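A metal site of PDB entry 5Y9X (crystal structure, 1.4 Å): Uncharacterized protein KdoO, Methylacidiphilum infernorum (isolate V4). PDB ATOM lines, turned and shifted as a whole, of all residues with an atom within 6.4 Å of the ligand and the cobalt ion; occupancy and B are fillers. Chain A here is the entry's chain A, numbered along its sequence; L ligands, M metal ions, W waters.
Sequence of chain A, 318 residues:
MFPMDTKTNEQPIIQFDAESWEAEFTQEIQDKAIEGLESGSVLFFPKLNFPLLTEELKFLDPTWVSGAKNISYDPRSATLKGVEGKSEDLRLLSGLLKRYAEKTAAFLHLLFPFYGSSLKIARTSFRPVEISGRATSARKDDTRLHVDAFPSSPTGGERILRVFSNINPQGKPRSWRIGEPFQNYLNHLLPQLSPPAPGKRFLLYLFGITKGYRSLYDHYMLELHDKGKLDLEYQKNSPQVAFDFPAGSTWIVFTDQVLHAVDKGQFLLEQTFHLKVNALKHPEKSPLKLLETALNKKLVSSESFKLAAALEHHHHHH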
ATOM      1  N   ARG A 127      17.661 -31.557   9.577  1.00  0.00           N
ATOM      2  CA  ARG A 127      16.576 -31.306   8.631  1.00  0.00           C
ATOM      3  C   ARG A 127      17.169 -30.925   7.286  1.00  0.00           C
ATOM      4  O   ARG A 127      17.438 -29.747   7.011  1.00  0.00           O
ATOM      5  CB  ARG A 127      15.621 -30.232   9.162  1.00  0.00           C
ATOM      6  CG  ARG A 127      15.214 -30.483  10.592  1.00  0.00           C
ATOM      7  CD  ARG A 127      14.233 -29.444  11.095  1.00  0.00           C
ATOM      8  NE  ARG A 127      13.808 -29.709  12.465  1.00  0.00           N
ATOM      9  CZ  ARG A 127      13.139 -28.830  13.205  1.00  0.00           C
ATOM     10  NH1 ARG A 127      12.816 -27.639  12.713  1.00  0.00           N
ATOM     11  NH2 ARG A 127      12.786 -29.146  14.444  1.00  0.00           N
ATOM     12  N   ILE A 131      12.376 -26.491   2.739  1.00  0.00           N
ATOM     13  CA  ILE A 131      11.076 -26.172   3.334  1.00  0.00           C
ATOM     14  C   ILE A 131      10.051 -25.789   2.257  1.00  0.00           C
ATOM     15  O   ILE A 131       8.869 -26.141   2.372  1.00  0.00           O
ATOM     16  CB  ILE A 131      11.236 -25.043   4.368  1.00  0.00           C
ATOM     17  CG1 ILE A 131      11.951 -25.564   5.612  1.00  0.00           C
ATOM     18  CG2 ILE A 131       9.879 -24.424   4.736  1.00  0.00           C
ATOM     19  CD1 ILE A 131      11.144 -26.539   6.420  1.00  0.00           C
ATOM     20  N   ASP A 142       4.109 -26.235   9.187  1.00  0.00           N
ATOM     21  CA  ASP A 142       4.837 -25.252   9.978  1.00  0.00           C
ATOM     22  C   ASP A 142       5.114 -23.954   9.230  1.00  0.00           C
ATOM     23  O   ASP A 142       5.863 -23.113   9.739  1.00  0.00           O
ATOM     24  CB  ASP A 142       6.093 -25.867  10.595  1.00  0.00           C
ATOM     25  CG  ASP A 142       5.779 -26.707  11.826  1.00  0.00           C
ATOM     26  OD1 ASP A 142       4.626 -26.662  12.314  1.00  0.00           O
ATOM     27  OD2 ASP A 142       6.689 -27.402  12.318  1.00  0.00           O
ATOM     28  N   HIS A 146       2.593 -20.952  15.024  1.00  0.00           N
ATOM     29  CA  HIS A 146       2.187 -21.854  16.086  1.00  0.00           C
ATOM     30  C   HIS A 146       3.181 -21.739  17.233  1.00  0.00           C
ATOM     31  O   HIS A 146       4.294 -21.238  17.069  1.00  0.00           O
ATOM     32  CB  HIS A 146       2.174 -23.296  15.575  1.00  0.00           C
ATOM     33  CG  HIS A 146       3.541 -23.781  15.199  1.00  0.00           C
ATOM     34  ND1 HIS A 146       4.153 -23.433  14.008  1.00  0.00           N
ATOM     35  CD2 HIS A 146       4.438 -24.543  15.872  1.00  0.00           C
ATOM     36  CE1 HIS A 146       5.365 -23.959  13.963  1.00  0.00           C
ATOM     37  NE2 HIS A 146       5.568 -24.643  15.088  1.00  0.00           N
ATOM     38  N   VAL A 147       2.749 -22.199  18.410  1.00  0.00           N
ATOM     39  CA  VAL A 147       3.659 -22.620  19.461  1.00  0.00           C
ATOM     40  C   VAL A 147       3.779 -24.134  19.388  1.00  0.00           C
ATOM     41  O   VAL A 147       2.869 -24.826  18.898  1.00  0.00           O
ATOM     42  CB  VAL A 147       3.213 -22.165  20.865  1.00  0.00           C
ATOM     43  CG1 VAL A 147       3.197 -20.660  20.946  1.00  0.00           C
ATOM     44  CG2 VAL A 147       1.856 -22.769  21.226  1.00  0.00           C
ATOM     45  N   ASP A 148       4.901 -24.666  19.849  1.00  0.00           N
ATOM     46  CA  ASP A 148       5.170 -26.096  19.715  1.00  0.00           C
ATOM     47  C   ASP A 148       4.351 -26.899  20.715  1.00  0.00           C
ATOM     48  O   ASP A 148       4.318 -26.600  21.912  1.00  0.00           O
ATOM     49  CB  ASP A 148       6.650 -26.396  19.896  1.00  0.00           C
ATOM     50  CG  ASP A 148       7.464 -26.084  18.657  1.00  0.00           C
ATOM     51  OD1 ASP A 148       6.876 -25.724  17.607  1.00  0.00           O
ATOM     52  OD2 ASP A 148       8.696 -26.207  18.749  1.00  0.00           O
ATOM     53  N   PHE A 150       3.105 -31.269  20.656  1.00  0.00           N
ATOM     54  CA  PHE A 150       3.205 -32.472  19.852  1.00  0.00           C
ATOM     55  C   PHE A 150       2.240 -33.509  20.411  1.00  0.00           C
ATOM     56  O   PHE A 150       2.362 -33.895  21.588  1.00  0.00           O
ATOM     57  CB  PHE A 150       4.651 -32.981  19.852  1.00  0.00           C
ATOM     58  CG  PHE A 150       5.614 -31.954  19.352  1.00  0.00           C
ATOM     59  CD1 PHE A 150       5.706 -31.666  17.999  1.00  0.00           C
ATOM     60  CD2 PHE A 150       6.402 -31.221  20.234  1.00  0.00           C
ATOM     61  CE1 PHE A 150       6.577 -30.698  17.525  1.00  0.00           C
ATOM     62  CE2 PHE A 150       7.278 -30.248  19.768  1.00  0.00           C
ATOM     63  CZ  PHE A 150       7.368 -29.997  18.412  1.00  0.00           C
ATOM     64  N   ARG A 162      14.515 -24.499  22.302  1.00  0.00           N
ATOM     65  CA  ARG A 162      15.185 -25.007  21.110  1.00  0.00           C
ATOM     66  C   ARG A 162      16.330 -24.115  20.688  1.00  0.00           C
ATOM     67  O   ARG A 162      16.224 -22.876  20.722  1.00  0.00           O
ATOM     68  CB  ARG A 162      14.199 -25.246  19.967  1.00  0.00           C
ATOM     69  CG  ARG A 162      13.205 -26.350  20.282  1.00  0.00           C
ATOM     70  CD  ARG A 162      12.318 -26.742  19.107  1.00  0.00           C
ATOM     71  NE  ARG A 162      11.952 -28.150  19.212  1.00  0.00           N
ATOM     72  CZ  ARG A 162      11.199 -28.822  18.351  1.00  0.00           C
ATOM     73  NH1 ARG A 162      10.670 -28.204  17.292  1.00  0.00           N
ATOM     74  NH2 ARG A 162      10.970 -30.116  18.541  1.00  0.00           N
ATOM     75  N   PHE A 164      18.809 -23.560  17.300  1.00  0.00           N
ATOM     76  CA  PHE A 164      18.751 -23.798  15.857  1.00  0.00           C
ATOM     77  C   PHE A 164      20.027 -23.259  15.241  1.00  0.00           C
ATOM     78  O   PHE A 164      20.500 -22.186  15.619  1.00  0.00           O
ATOM     79  CB  PHE A 164      17.609 -22.987  15.237  1.00  0.00           C
ATOM     80  CG  PHE A 164      16.237 -23.411  15.643  1.00  0.00           C
ATOM     81  CD1 PHE A 164      15.586 -22.815  16.718  1.00  0.00           C
ATOM     82  CD2 PHE A 164      15.565 -24.391  14.921  1.00  0.00           C
ATOM     83  CE1 PHE A 164      14.290 -23.188  17.059  1.00  0.00           C
ATOM     84  CE2 PHE A 164      14.273 -24.772  15.264  1.00  0.00           C
ATOM     85  CZ  PHE A 164      13.634 -24.169  16.340  1.00  0.00           C
ATOM     86  N   ARG A 174      17.375 -19.064   6.320  1.00  0.00           N
ATOM     87  CA  ARG A 174      16.191 -19.786   6.754  1.00  0.00           C
ATOM     88  C   ARG A 174      15.144 -18.744   7.097  1.00  0.00           C
ATOM     89  O   ARG A 174      15.335 -17.944   8.023  1.00  0.00           O
ATOM     90  CB  ARG A 174      16.481 -20.703   7.930  1.00  0.00           C
ATOM     91  CG  ARG A 174      15.378 -21.739   8.110  1.00  0.00           C
ATOM     92  CD  ARG A 174      15.876 -22.951   8.772  1.00  0.00           C
ATOM     93  NE  ARG A 174      14.930 -24.056   8.834  1.00  0.00           N
ATOM     94  CZ  ARG A 174      14.945 -25.120   8.022  1.00  0.00           C
ATOM     95  NH1 ARG A 174      15.843 -25.201   7.051  1.00  0.00           N
ATOM     96  NH2 ARG A 174      14.076 -26.104   8.200  1.00  0.00           N
ATOM     97  N   SER A 175      14.058 -18.730   6.336  1.00  0.00           N
ATOM     98  CA  SER A 175      13.075 -17.647   6.417  1.00  0.00           C
ATOM     99  C   SER A 175      12.016 -18.011   7.453  1.00  0.00           C
ATOM    100  O   SER A 175      11.249 -18.962   7.246  1.00  0.00           O
ATOM    101  CB  SER A 175      12.445 -17.403   5.054  1.00  0.00           C
ATOM    102  OG  SER A 175      13.422 -16.941   4.125  1.00  0.00           O
ATOM    103  N   TRP A 176      11.984 -17.273   8.554  1.00  0.00           N
ATOM    104  CA  TRP A 176      10.990 -17.432   9.597  1.00  0.00           C
ATOM    105  C   TRP A 176      10.008 -16.264   9.586  1.00  0.00           C
ATOM    106  O   TRP A 176      10.278 -15.188   9.056  1.00  0.00           O
ATOM    107  CB  TRP A 176      11.661 -17.471  10.969  1.00  0.00           C
ATOM    108  CG  TRP A 176      12.025 -18.840  11.464  1.00  0.00           C
ATOM    109  CD1 TRP A 176      12.406 -19.913  10.714  1.00  0.00           C
ATOM    110  CD2 TRP A 176      12.030 -19.272  12.821  1.00  0.00           C
ATOM    111  NE1 TRP A 176      12.670 -20.993  11.542  1.00  0.00           N
ATOM    112  CE2 TRP A 176      12.425 -20.626  12.840  1.00  0.00           C
ATOM    113  CE3 TRP A 176      11.729 -18.637  14.041  1.00  0.00           C
ATOM    114  CZ2 TRP A 176      12.530 -21.365  14.019  1.00  0.00           C
ATOM    115  CZ3 TRP A 176      11.829 -19.368  15.218  1.00  0.00           C
ATOM    116  CH2 TRP A 176      12.220 -20.721  15.200  1.00  0.00           C
ATOM    117  N   HIS A 225      -2.214 -24.652  19.305  1.00  0.00           N
ATOM    118  CA  HIS A 225      -1.448 -24.993  18.125  1.00  0.00           C
ATOM    119  C   HIS A 225      -2.368 -25.289  16.937  1.00  0.00           C
ATOM    120  O   HIS A 225      -2.256 -24.667  15.870  1.00  0.00           O
ATOM    121  CB  HIS A 225      -0.582 -26.226  18.470  1.00  0.00           C
ATOM    122  CG  HIS A 225       0.163 -26.823  17.313  1.00  0.00           C
ATOM    123  ND1 HIS A 225      -0.443 -27.670  16.404  1.00  0.00           N
ATOM    124  CD2 HIS A 225       1.469 -26.747  16.949  1.00  0.00           C
ATOM    125  CE1 HIS A 225       0.462 -28.079  15.523  1.00  0.00           C
ATOM    126  NE2 HIS A 225       1.621 -27.526  15.828  1.00  0.00           N
ATOM    127  N   TRP A 251      20.181 -19.503  16.590  1.00  0.00           N
ATOM    128  CA  TRP A 251      19.205 -18.788  17.392  1.00  0.00           C
ATOM    129  C   TRP A 251      18.605 -19.699  18.445  1.00  0.00           C
ATOM    130  O   TRP A 251      18.630 -20.925  18.320  1.00  0.00           O
ATOM    131  CB  TRP A 251      18.155 -18.067  16.534  1.00  0.00           C
ATOM    132  CG  TRP A 251      17.302 -18.918  15.619  1.00  0.00           C
ATOM    133  CD1 TRP A 251      15.984 -19.238  15.796  1.00  0.00           C
ATOM    134  CD2 TRP A 251      17.683 -19.484  14.347  1.00  0.00           C
ATOM    135  NE1 TRP A 251      15.528 -19.989  14.737  1.00  0.00           N
ATOM    136  CE2 TRP A 251      16.543 -20.150  13.836  1.00  0.00           C
ATOM    137  CE3 TRP A 251      18.868 -19.492  13.606  1.00  0.00           C
ATOM    138  CZ2 TRP A 251      16.563 -20.830  12.616  1.00  0.00           C
ATOM    139  CZ3 TRP A 251      18.880 -20.162  12.398  1.00  0.00           C
ATOM    140  CH2 TRP A 251      17.735 -20.824  11.914  1.00  0.00           C
ATOM    141  N   THR A 255      10.126 -22.337  22.038  1.00  0.00           N
ATOM    142  CA  THR A 255       9.175 -22.476  20.932  1.00  0.00           C
ATOM    143  C   THR A 255       7.763 -22.835  21.401  1.00  0.00           C
ATOM    144  O   THR A 255       6.834 -22.793  20.580  1.00  0.00           O
ATOM    145  CB  THR A 255       9.660 -23.507  19.920  1.00  0.00           C
ATOM    146  OG1 THR A 255       9.935 -24.725  20.602  1.00  0.00           O
ATOM    147  CG2 THR A 255      10.906 -23.022  19.211  1.00  0.00           C
ATOM    148  N   HIS A 260       5.900 -18.974  15.860  1.00  0.00           N
ATOM    149  CA  HIS A 260       6.888 -19.048  14.804  1.00  0.00           C
ATOM    150  C   HIS A 260       6.333 -19.849  13.637  1.00  0.00           C
ATOM    151  O   HIS A 260       5.363 -20.617  13.771  1.00  0.00           O
ATOM    152  CB  HIS A 260       8.208 -19.641  15.314  1.00  0.00           C
ATOM    153  CG  HIS A 260       8.052 -21.027  15.859  1.00  0.00           C
ATOM    154  ND1 HIS A 260       7.485 -21.279  17.096  1.00  0.00           N
ATOM    155  CD2 HIS A 260       8.308 -22.237  15.321  1.00  0.00           C
ATOM    156  CE1 HIS A 260       7.414 -22.586  17.291  1.00  0.00           C
ATOM    157  NE2 HIS A 260       7.919 -23.191  16.232  1.00  0.00           N
ATOM    158  N   ALA A 261       6.958 -19.651  12.477  1.00  0.00           N
ATOM    159  CA  ALA A 261       6.658 -20.366  11.248  1.00  0.00           C
ATOM    160  C   ALA A 261       7.902 -20.293  10.369  1.00  0.00           C
ATOM    161  O   ALA A 261       8.705 -19.373  10.507  1.00  0.00           O
ATOM    162  CB  ALA A 261       5.486 -19.724  10.499  1.00  0.00           C
ATOM    163  N   VAL A 262       8.063 -21.268   9.480  1.00  0.00           N
ATOM    164  CA  VAL A 262       9.183 -21.268   8.550  1.00  0.00           C
ATOM    165  C   VAL A 262       8.639 -21.344   7.132  1.00  0.00           C
ATOM    166  O   VAL A 262       7.730 -22.147   6.854  1.00  0.00           O
ATOM    167  CB  VAL A 262      10.189 -22.395   8.851  1.00  0.00           C
ATOM    168  CG1 VAL A 262       9.525 -23.765   8.810  1.00  0.00           C
ATOM    169  CG2 VAL A 262      11.390 -22.319   7.891  1.00  0.00           C
ATOM    170  N   LEU A 268      19.322 -27.626   8.412  1.00  0.00           N
ATOM    171  CA  LEU A 268      19.184 -27.046   9.738  1.00  0.00           C
ATOM    172  C   LEU A 268      19.529 -28.115  10.749  1.00  0.00           C
ATOM    173  O   LEU A 268      19.124 -29.277  10.608  1.00  0.00           O
ATOM    174  CB  LEU A 268      17.714 -26.624   9.964  1.00  0.00           C
ATOM    175  CG  LEU A 268      17.364 -25.956  11.286  1.00  0.00           C
ATOM    176  CD1 LEU A 268      17.831 -24.518  11.299  1.00  0.00           C
ATOM    177  CD2 LEU A 268      15.854 -26.051  11.575  1.00  0.00           C
ATOM    178  N   GLU A 270      18.968 -28.721  14.891  1.00  0.00           N
ATOM    179  CA  GLU A 270      18.118 -28.233  15.954  1.00  0.00           C
ATOM    180  C   GLU A 270      18.316 -29.120  17.179  1.00  0.00           C
ATOM    181  O   GLU A 270      18.465 -30.345  17.058  1.00  0.00           O
ATOM    182  CB  GLU A 270      16.648 -28.198  15.505  1.00  0.00           C
ATOM    183  CG  GLU A 270      15.643 -27.756  16.558  1.00  0.00           C
ATOM    184  CD  GLU A 270      15.167 -28.901  17.427  1.00  0.00           C
ATOM    185  OE1 GLU A 270      15.014 -30.034  16.919  1.00  0.00           O
ATOM    186  OE2 GLU A 270      14.958 -28.669  18.627  1.00  0.00           O
HETATM  187  C1  LIG L   1      10.116 -25.952  14.802  1.00  0.00           C
HETATM  188  O1  LIG L   1      11.275 -26.455  14.735  1.00  0.00           O
HETATM  189  O2  LIG L   1       9.487 -25.898  15.890  1.00  0.00           O
HETATM  190  C2  LIG L   1       9.459 -25.418  13.568  1.00  0.00           C
HETATM  191  O3  LIG L   1       8.313 -24.964  13.644  1.00  0.00           O
HETATM  192  C3  LIG L   1      10.189 -25.407  12.273  1.00  0.00           C
HETATM  193  C4  LIG L   1      11.291 -24.411  12.170  1.00  0.00           C
HETATM  194  C5  LIG L   1      12.258 -24.617  11.063  1.00  0.00           C
HETATM  195  O4  LIG L   1      12.310 -25.726  10.454  1.00  0.00           O
HETATM  196  O5  LIG L   1      13.049 -23.695  10.732  1.00  0.00           O
HETATM  197 CO    CO M   1       7.535 -25.228  15.729  1.00  0.00          CO
HETATM  198  O   HOH W   1      10.444 -27.679   9.718  1.00  0.00           O
HETATM  199  O   HOH W   2       6.982 -27.299  15.152  1.00  0.00           O
HETATM  200  O   HOH W   3       9.027 -28.654  11.873  1.00  0.00           O
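The guanidinium group (NE) of Arg 174 lies within salt-bridge range of an oxygen (O5) of the ligand, 2.7 Å away.
The guanidinium group of Arg 127 lies within salt-bridge range of an oxygen (O1) of the ligand.
The indole nitrogen (NE1) of Trp 176 is in hydrogen-bond range of an oxygen (O5) of the ligand (2.8 Å).
The guanidinium group (NH1) of Arg 162 is in salt-bridge range of an oxygen (O1) of the ligand, at 3.2 Å.
The side-chain carboxylate (OD2) of Asp 148 lies within salt-bridge range of the guanidinium group (NH1) of Arg 162 (3.2 Å).
OD2 of Asp 148 lies within hydrogen-bond range of OG1 of Thr 255 (2.7 Å).
The backbone NH (N) of Arg 127 sits at hydrogen-bond distance from the backbone carbonyl oxygen (O) of Leu 268, at 2.9 Å.
The guanidinium group (NH2) of Arg 127 lies within salt-bridge range of the side-chain carboxylate (OE1) of Glu 270.
OE2 of Glu 270 lies within salt-bridge range of NE of Arg 162 (3.1 Å).
N of Val 262 is in hydrogen-bond range of O of Asp 142 (2.9 Å).
N of Phe 164 is in hydrogen-bond range of O of Trp 251, 2.8 Å away.
The side-chain carboxylate of Asp 142 lies close to an oxygen (O3) of the ligand (3.2 Å).
Residues that only touch the ligand: Phe 164 (3.5 Å), Val 262 (3.6 Å) and Leu 268 (3.7 Å).
Hydrophobic or aromatic side chains that line the ligand: His 146, Phe 164, Trp 176, His 260, Val 262 and Leu 268.
Within 4 Å of the ligand: Arg 127, Asp 142, His 146, Asp 148, Arg 162, Phe 164, Arg 174, Trp 176, His 260, Val 262 and Leu 268.
Along chain A the residues within 4 Å of the ligand span positions 127 to 268.
Within 4 Å of the cobalt ion: His 146, Asp 148 and His 260.
The nearest printed residue that does not touch the cobalt ion is Asp 142 (4.1 Å).
The cobalt ion is bound by OD1 of Asp 148 (2.1 Å), O2 of the ligand (2.1 Å), NE2 of His 260 (2.1 Å), NE2 of His 146 (2.1 Å), water W2 (2.2 Å) and O3 of the ligand (2.2 Å).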
